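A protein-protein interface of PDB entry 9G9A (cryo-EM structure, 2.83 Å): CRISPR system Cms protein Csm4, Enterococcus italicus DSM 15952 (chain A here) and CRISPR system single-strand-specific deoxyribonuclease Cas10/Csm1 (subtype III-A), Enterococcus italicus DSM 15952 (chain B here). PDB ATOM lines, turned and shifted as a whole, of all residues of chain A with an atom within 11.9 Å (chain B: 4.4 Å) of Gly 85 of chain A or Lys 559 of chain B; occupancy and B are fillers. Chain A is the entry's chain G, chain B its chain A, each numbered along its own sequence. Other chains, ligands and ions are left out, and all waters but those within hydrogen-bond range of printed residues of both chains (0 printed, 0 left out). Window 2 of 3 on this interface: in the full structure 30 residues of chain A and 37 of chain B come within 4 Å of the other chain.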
ATOM      1  N   ILE A  80      -3.583  -9.700 -11.295  1.00  0.00           N
ATOM      2  CA  ILE A  80      -2.638 -10.691 -11.795  1.00  0.00           C
ATOM      3  C   ILE A  80      -2.153 -10.237 -13.164  1.00  0.00           C
ATOM      4  O   ILE A  80      -2.960 -10.012 -14.074  1.00  0.00           O
ATOM      5  CB  ILE A  80      -3.277 -12.086 -11.868  1.00  0.00           C
ATOM      6  CG1 ILE A  80      -3.732 -12.533 -10.478  1.00  0.00           C
ATOM      7  CG2 ILE A  80      -2.302 -13.087 -12.460  1.00  0.00           C
ATOM      8  CD1 ILE A  80      -4.413 -13.878 -10.464  1.00  0.00           C
ATOM      9  N   GLU A  81      -0.833 -10.100 -13.313  1.00  0.00           N
ATOM     10  CA  GLU A  81      -0.278  -9.654 -14.588  1.00  0.00           C
ATOM     11  C   GLU A  81      -0.461 -10.710 -15.672  1.00  0.00           C
ATOM     12  O   GLU A  81      -0.684 -10.373 -16.841  1.00  0.00           O
ATOM     13  CB  GLU A  81       1.200  -9.289 -14.426  1.00  0.00           C
ATOM     14  CG  GLU A  81       2.129 -10.449 -14.079  1.00  0.00           C
ATOM     15  CD  GLU A  81       2.082 -10.838 -12.612  1.00  0.00           C
ATOM     16  OE1 GLU A  81       1.322 -10.208 -11.846  1.00  0.00           O
ATOM     17  OE2 GLU A  81       2.810 -11.777 -12.226  1.00  0.00           O
ATOM     18  N   GLY A  82      -0.375 -11.986 -15.308  1.00  0.00           N
ATOM     19  CA  GLY A  82      -0.546 -13.064 -16.264  1.00  0.00           C
ATOM     20  C   GLY A  82       0.603 -13.197 -17.244  1.00  0.00           C
ATOM     21  O   GLY A  82       1.590 -12.467 -17.163  1.00  0.00           O
ATOM     22  N   GLY A  85      -0.416 -13.735 -23.194  1.00  0.00           N
ATOM     23  CA  GLY A  85      -0.609 -14.439 -24.448  1.00  0.00           C
ATOM     24  C   GLY A  85      -1.739 -15.447 -24.403  1.00  0.00           C
ATOM     25  O   GLY A  85      -2.239 -15.877 -25.443  1.00  0.00           O
ATOM     26  N   ASP A  86      -2.142 -15.832 -23.193  1.00  0.00           N
ATOM     27  CA  ASP A  86      -3.216 -16.799 -22.987  1.00  0.00           C
ATOM     28  C   ASP A  86      -4.244 -16.198 -22.040  1.00  0.00           C
ATOM     29  O   ASP A  86      -3.927 -15.891 -20.886  1.00  0.00           O
ATOM     30  CB  ASP A  86      -2.671 -18.119 -22.439  1.00  0.00           C
ATOM     31  CG  ASP A  86      -1.446 -17.929 -21.566  1.00  0.00           C
ATOM     32  OD1 ASP A  86      -1.581 -17.374 -20.456  1.00  0.00           O
ATOM     33  OD2 ASP A  86      -0.345 -18.335 -21.995  1.00  0.00           O
ATOM     34  N   GLU A  87      -5.475 -16.023 -22.530  1.00  0.00           N
ATOM     35  CA  GLU A  87      -6.537 -15.485 -21.687  1.00  0.00           C
ATOM     36  C   GLU A  87      -7.137 -16.565 -20.795  1.00  0.00           C
ATOM     37  O   GLU A  87      -7.723 -16.259 -19.750  1.00  0.00           O
ATOM     38  CB  GLU A  87      -7.618 -14.841 -22.555  1.00  0.00           C
ATOM     39  CG  GLU A  87      -7.142 -13.623 -23.328  1.00  0.00           C
ATOM     40  CD  GLU A  87      -6.775 -12.466 -22.421  1.00  0.00           C
ATOM     41  OE1 GLU A  87      -7.653 -11.996 -21.666  1.00  0.00           O
ATOM     42  OE2 GLU A  87      -5.605 -12.032 -22.454  1.00  0.00           O
ATOM     43  N   SER A  88      -7.003 -17.833 -21.190  1.00  0.00           N
ATOM     44  CA  SER A  88      -7.537 -18.925 -20.385  1.00  0.00           C
ATOM     45  C   SER A  88      -6.795 -19.083 -19.065  1.00  0.00           C
ATOM     46  O   SER A  88      -7.344 -19.658 -18.117  1.00  0.00           O
ATOM     47  CB  SER A  88      -7.486 -20.234 -21.179  1.00  0.00           C
ATOM     48  OG  SER A  88      -6.166 -20.521 -21.605  1.00  0.00           O
ATOM     49  N   GLY A  89      -5.558 -18.590 -18.982  1.00  0.00           N
ATOM     50  CA  GLY A  89      -4.860 -18.593 -17.707  1.00  0.00           C
ATOM     51  C   GLY A  89      -5.569 -17.755 -16.663  1.00  0.00           C
ATOM     52  O   GLY A  89      -5.622 -18.122 -15.485  1.00  0.00           O
ATOM     53  N   TYR A  90      -6.128 -16.619 -17.080  1.00  0.00           N
ATOM     54  CA  TYR A  90      -6.925 -15.815 -16.163  1.00  0.00           C
ATOM     55  C   TYR A  90      -8.171 -16.563 -15.711  1.00  0.00           C
ATOM     56  O   TYR A  90      -8.595 -16.418 -14.561  1.00  0.00           O
ATOM     57  CB  TYR A  90      -7.297 -14.487 -16.819  1.00  0.00           C
ATOM     58  CG  TYR A  90      -6.093 -13.681 -17.245  1.00  0.00           C
ATOM     59  CD1 TYR A  90      -5.324 -13.000 -16.311  1.00  0.00           C
ATOM     60  CD2 TYR A  90      -5.723 -13.605 -18.579  1.00  0.00           C
ATOM     61  CE1 TYR A  90      -4.221 -12.263 -16.695  1.00  0.00           C
ATOM     62  CE2 TYR A  90      -4.621 -12.871 -18.973  1.00  0.00           C
ATOM     63  CZ  TYR A  90      -3.875 -12.202 -18.027  1.00  0.00           C
ATOM     64  OH  TYR A  90      -2.776 -11.471 -18.414  1.00  0.00           O
ATOM     65  N   LYS A  91      -8.761 -17.376 -16.589  1.00  0.00           N
ATOM     66  CA  LYS A  91      -9.882 -18.216 -16.177  1.00  0.00           C
ATOM     67  C   LYS A  91      -9.443 -19.249 -15.146  1.00  0.00           C
ATOM     68  O   LYS A  91     -10.165 -19.518 -14.175  1.00  0.00           O
ATOM     69  CB  LYS A  91     -10.498 -18.895 -17.400  1.00  0.00           C
ATOM     70  CG  LYS A  91     -11.645 -19.839 -17.086  1.00  0.00           C
ATOM     71  CD  LYS A  91     -12.405 -20.210 -18.348  1.00  0.00           C
ATOM     72  CE  LYS A  91     -11.476 -20.770 -19.412  1.00  0.00           C
ATOM     73  NZ  LYS A  91     -12.195 -21.036 -20.688  1.00  0.00           N
ATOM     74  N   PHE A  93      -6.997 -18.891 -13.023  1.00  0.00           N
ATOM     75  CA  PHE A  93      -6.872 -18.137 -11.777  1.00  0.00           C
ATOM     76  C   PHE A  93      -8.239 -17.846 -11.169  1.00  0.00           C
ATOM     77  O   PHE A  93      -8.400 -17.874  -9.943  1.00  0.00           O
ATOM     78  CB  PHE A  93      -6.114 -16.832 -12.015  1.00  0.00           C
ATOM     79  CG  PHE A  93      -4.627 -17.001 -12.128  1.00  0.00           C
ATOM     80  CD1 PHE A  93      -3.873 -17.355 -11.023  1.00  0.00           C
ATOM     81  CD2 PHE A  93      -3.981 -16.785 -13.332  1.00  0.00           C
ATOM     82  CE1 PHE A  93      -2.507 -17.503 -11.122  1.00  0.00           C
ATOM     83  CE2 PHE A  93      -2.616 -16.934 -13.437  1.00  0.00           C
ATOM     84  CZ  PHE A  93      -1.878 -17.292 -12.331  1.00  0.00           C
ATOM     85  N   ASP A 113       1.842 -19.522 -11.394  1.00  0.00           N
ATOM     86  CA  ASP A 113       1.381 -19.481 -12.772  1.00  0.00           C
ATOM     87  C   ASP A 113      -0.011 -20.101 -12.886  1.00  0.00           C
ATOM     88  O   ASP A 113      -0.555 -20.658 -11.929  1.00  0.00           O
ATOM     89  CB  ASP A 113       2.373 -20.202 -13.685  1.00  0.00           C
ATOM     90  CG  ASP A 113       2.251 -19.776 -15.135  1.00  0.00           C
ATOM     91  OD1 ASP A 113       1.324 -19.002 -15.455  1.00  0.00           O
ATOM     92  OD2 ASP A 113       3.084 -20.214 -15.954  1.00  0.00           O
ATOM     93  N   SER A 114      -0.592 -19.994 -14.084  1.00  0.00           N
ATOM     94  CA  SER A 114      -1.938 -20.514 -14.306  1.00  0.00           C
ATOM     95  C   SER A 114      -1.990 -22.024 -14.116  1.00  0.00           C
ATOM     96  O   SER A 114      -2.927 -22.549 -13.502  1.00  0.00           O
ATOM     97  CB  SER A 114      -2.421 -20.135 -15.704  1.00  0.00           C
ATOM     98  OG  SER A 114      -1.556 -20.649 -16.699  1.00  0.00           O
ATOM     99  N   LEU A 115      -0.995 -22.742 -14.641  1.00  0.00           N
ATOM    100  CA  LEU A 115      -0.921 -24.179 -14.402  1.00  0.00           C
ATOM    101  C   LEU A 115      -0.708 -24.471 -12.923  1.00  0.00           C
ATOM    102  O   LEU A 115      -1.323 -25.390 -12.369  1.00  0.00           O
ATOM    103  CB  LEU A 115       0.194 -24.801 -15.242  1.00  0.00           C
ATOM    104  CG  LEU A 115      -0.158 -25.249 -16.665  1.00  0.00           C
ATOM    105  CD1 LEU A 115      -1.282 -26.275 -16.640  1.00  0.00           C
ATOM    106  CD2 LEU A 115      -0.522 -24.067 -17.556  1.00  0.00           C
ATOM    107  N   ASN B 139      -4.039 -21.316 -35.218  1.00  0.00           N
ATOM    108  CA  ASN B 139      -3.257 -22.414 -34.650  1.00  0.00           C
ATOM    109  C   ASN B 139      -2.311 -23.045 -35.669  1.00  0.00           C
ATOM    110  O   ASN B 139      -1.958 -24.222 -35.544  1.00  0.00           O
ATOM    111  CB  ASN B 139      -4.168 -23.487 -34.041  1.00  0.00           C
ATOM    112  CG  ASN B 139      -4.940 -22.982 -32.837  1.00  0.00           C
ATOM    113  OD1 ASN B 139      -4.514 -22.047 -32.158  1.00  0.00           O
ATOM    114  ND2 ASN B 139      -6.080 -23.604 -32.563  1.00  0.00           N
ATOM    115  N   GLU B 141       0.727 -22.329 -36.055  1.00  0.00           N
ATOM    116  CA  GLU B 141       2.043 -22.487 -35.449  1.00  0.00           C
ATOM    117  C   GLU B 141       2.268 -23.910 -34.956  1.00  0.00           C
ATOM    118  O   GLU B 141       3.413 -24.367 -34.874  1.00  0.00           O
ATOM    119  CB  GLU B 141       2.215 -21.500 -34.292  1.00  0.00           C
ATOM    120  CG  GLU B 141       1.997 -20.045 -34.666  1.00  0.00           C
ATOM    121  CD  GLU B 141       0.808 -19.436 -33.950  1.00  0.00           C
ATOM    122  OE1 GLU B 141      -0.130 -20.188 -33.611  1.00  0.00           O
ATOM    123  OE2 GLU B 141       0.813 -18.208 -33.721  1.00  0.00           O
ATOM    124  N   GLN B 391      -5.774  -7.378 -24.742  1.00  0.00           N
ATOM    125  CA  GLN B 391      -5.487  -7.800 -23.375  1.00  0.00           C
ATOM    126  C   GLN B 391      -5.608  -6.638 -22.399  1.00  0.00           C
ATOM    127  O   GLN B 391      -6.087  -6.813 -21.274  1.00  0.00           O
ATOM    128  CB  GLN B 391      -4.097  -8.429 -23.302  1.00  0.00           C
ATOM    129  CG  GLN B 391      -3.999  -9.770 -24.003  1.00  0.00           C
ATOM    130  CD  GLN B 391      -2.618 -10.381 -23.908  1.00  0.00           C
ATOM    131  OE1 GLN B 391      -1.647  -9.702 -23.574  1.00  0.00           O
ATOM    132  NE2 GLN B 391      -2.523 -11.672 -24.199  1.00  0.00           N
ATOM    133  N   THR B 555      -7.615 -17.518 -25.797  1.00  0.00           N
ATOM    134  CA  THR B 555      -6.230 -17.716 -26.213  1.00  0.00           C
ATOM    135  C   THR B 555      -6.133 -17.896 -27.723  1.00  0.00           C
ATOM    136  O   THR B 555      -5.209 -17.377 -28.360  1.00  0.00           O
ATOM    137  CB  THR B 555      -5.633 -18.920 -25.483  1.00  0.00           C
ATOM    138  OG1 THR B 555      -5.811 -18.761 -24.070  1.00  0.00           O
ATOM    139  CG2 THR B 555      -4.152 -19.050 -25.783  1.00  0.00           C
ATOM    140  N   THR B 556      -7.082 -18.626 -28.314  1.00  0.00           N
ATOM    141  CA  THR B 556      -7.104 -18.776 -29.766  1.00  0.00           C
ATOM    142  C   THR B 556      -7.317 -17.432 -30.452  1.00  0.00           C
ATOM    143  O   THR B 556      -6.711 -17.154 -31.494  1.00  0.00           O
ATOM    144  CB  THR B 556      -8.192 -19.767 -30.179  1.00  0.00           C
ATOM    145  OG1 THR B 556      -7.994 -21.008 -29.491  1.00  0.00           O
ATOM    146  CG2 THR B 556      -8.146 -20.021 -31.680  1.00  0.00           C
ATOM    147  N   PHE B 557      -8.181 -16.587 -29.887  1.00  0.00           N
ATOM    148  CA  PHE B 557      -8.342 -15.238 -30.420  1.00  0.00           C
ATOM    149  C   PHE B 557      -7.041 -14.449 -30.325  1.00  0.00           C
ATOM    150  O   PHE B 557      -6.660 -13.744 -31.267  1.00  0.00           O
ATOM    151  CB  PHE B 557      -9.465 -14.508 -29.682  1.00  0.00           C
ATOM    152  CG  PHE B 557     -10.822 -14.698 -30.295  1.00  0.00           C
ATOM    153  CD1 PHE B 557     -11.221 -13.924 -31.372  1.00  0.00           C
ATOM    154  CD2 PHE B 557     -11.701 -15.639 -29.789  1.00  0.00           C
ATOM    155  CE1 PHE B 557     -12.469 -14.092 -31.937  1.00  0.00           C
ATOM    156  CE2 PHE B 557     -12.951 -15.809 -30.350  1.00  0.00           C
ATOM    157  CZ  PHE B 557     -13.334 -15.035 -31.426  1.00  0.00           C
ATOM    158  N   ILE B 558      -6.344 -14.558 -29.192  1.00  0.00           N
ATOM    159  CA  ILE B 558      -5.165 -13.725 -28.962  1.00  0.00           C
ATOM    160  C   ILE B 558      -3.967 -14.240 -29.751  1.00  0.00           C
ATOM    161  O   ILE B 558      -3.288 -13.473 -30.443  1.00  0.00           O
ATOM    162  CB  ILE B 558      -4.860 -13.637 -27.456  1.00  0.00           C
ATOM    163  CG1 ILE B 558      -5.987 -12.903 -26.729  1.00  0.00           C
ATOM    164  CG2 ILE B 558      -3.529 -12.940 -27.220  1.00  0.00           C
ATOM    165  CD1 ILE B 558      -6.240 -11.505 -27.248  1.00  0.00           C
ATOM    166  N   LYS B 559      -3.684 -15.542 -29.665  1.00  0.00           N
ATOM    167  CA  LYS B 559      -2.476 -16.092 -30.275  1.00  0.00           C
ATOM    168  C   LYS B 559      -2.724 -17.152 -31.336  1.00  0.00           C
ATOM    169  O   LYS B 559      -1.763 -17.543 -32.011  1.00  0.00           O
ATOM    170  CB  LYS B 559      -1.549 -16.684 -29.198  1.00  0.00           C
ATOM    171  CG  LYS B 559      -2.093 -17.921 -28.491  1.00  0.00           C
ATOM    172  CD  LYS B 559      -1.586 -19.216 -29.116  1.00  0.00           C
ATOM    173  CE  LYS B 559      -2.479 -20.390 -28.750  1.00  0.00           C
ATOM    174  NZ  LYS B 559      -2.117 -21.625 -29.498  1.00  0.00           N
ATOM    175  N   GLY B 560      -3.955 -17.639 -31.506  1.00  0.00           N
ATOM    176  CA  GLY B 560      -4.201 -18.648 -32.526  1.00  0.00           C
ATOM    177  C   GLY B 560      -3.883 -18.146 -33.919  1.00  0.00           C
ATOM    178  O   GLY B 560      -3.259 -18.846 -34.721  1.00  0.00           O
ATOM    179  N   ILE B 561      -4.305 -16.924 -34.224  1.00  0.00           N
ATOM    180  CA  ILE B 561      -3.942 -16.265 -35.474  1.00  0.00           C
ATOM    181  C   ILE B 561      -2.528 -15.716 -35.321  1.00  0.00           C
ATOM    182  O   ILE B 561      -2.259 -14.962 -34.374  1.00  0.00           O
ATOM    183  CB  ILE B 561      -4.944 -15.158 -35.834  1.00  0.00           C
ATOM    184  CG1 ILE B 561      -6.363 -15.726 -35.903  1.00  0.00           C
ATOM    185  CG2 ILE B 561      -4.572 -14.512 -37.155  1.00  0.00           C
ATOM    186  CD1 ILE B 561      -7.419 -14.699 -36.251  1.00  0.00           C
ATOM    187  N   ARG B 566      -2.703 -11.574 -37.821  1.00  0.00           N
ATOM    188  CA  ARG B 566      -3.613 -10.933 -36.879  1.00  0.00           C
ATOM    189  C   ARG B 566      -3.957  -9.517 -37.323  1.00  0.00           C
ATOM    190  O   ARG B 566      -3.083  -8.741 -37.716  1.00  0.00           O
ATOM    191  CB  ARG B 566      -2.990 -10.910 -35.481  1.00  0.00           C
ATOM    192  CG  ARG B 566      -3.615 -11.898 -34.512  1.00  0.00           C
ATOM    193  CD  ARG B 566      -2.880 -11.915 -33.181  1.00  0.00           C
ATOM    194  NE  ARG B 566      -1.652 -12.698 -33.239  1.00  0.00           N
ATOM    195  CZ  ARG B 566      -0.828 -12.875 -32.214  1.00  0.00           C
ATOM    196  NH1 ARG B 566      -1.061 -12.322 -31.036  1.00  0.00           N
ATOM    197  NH2 ARG B 566       0.255 -13.631 -32.376  1.00  0.00           N
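The side-chain amide nitrogen of Gln 391 of chain B lies close to the backbone NH of Gly 85 of chain A, 3.1 Å away.
The side-chain hydroxyl (OG1) of Thr 555 of chain B lies within hydrogen-bond range of the backbone NH (N) of Glu 87 of chain A (3.2 Å).
The side-chain hydroxyl of Ser 88 of chain A lies within hydrogen-bond range of the side-chain hydroxyl of Thr 555 of chain B, at 3.0 Å.
The backbone carbonyl oxygen (O) of Thr 555 of chain B lies within hydrogen-bond range of the backbone NH (N) of Gly 560 of chain B.
The backbone carbonyl oxygen (O) of Ile 558 of chain B is in hydrogen-bond range of the guanidinium group (NH1) of Arg 566 of chain B (2.6 Å).
O of Gly 85 of chain A touches CG2 of Thr 555 of chain B, 3.7 Å away.
Gly 85 of chain A touches Ile 558 of chain B (O to CG2, 3.7 Å).
CG of Lys 559 of chain B touches O of Gly 85 of chain A, 3.7 Å away.
Thr 555 of chain B touches Asp 86 of chain A.
CG of Gln 391 of chain B touches OE2 of Glu 87 of chain A (3.2 Å).
CG of Glu 87 of chain A touches CG1 of Ile 558 of chain B, 3.7 Å away.
Printed residues of chain B within 4 Å of Gly 85 of chain A: Gln 391, Thr 555, Ile 558 and Lys 559.
Of chain A, only Gly 85 (3.7 Å) comes within 4 Å of Lys 559 of chain B.
No residue of chain A comes within 4 Å of Asn 139 of chain B.
Of the printed residues of chain A, Thr 555 of chain B touches Gly 85, Asp 86, Glu 87 and Ser 88.
No residue of chain A comes within 4 Å of Gly 560 of chain B.
Printed residues of chain B within 4 Å of Asp 86 of chain A: Thr 555 (3.4 Å).
Of the printed residues of chain B, Ser 88 of chain A touches Thr 555.
Of the printed residues of chain B, Glu 87 of chain A touches Gln 391, Thr 555 and Ile 558.
Lys 91 of chain A touches none of the printed residues of chain B.
Asp 113 of chain A touches none of the printed residues of chain B.
Of the 14 printed residues of chain A, 4 touch a printed residue of chain B.
Along chain A the printed residues that touch a printed residue of chain B span positions 85 to 88.
Hydrophobic or aromatic side chains of chain B that line the printed part of chain A: Ile 558.
Among the printed residues, 9 pairs touch across the chains.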
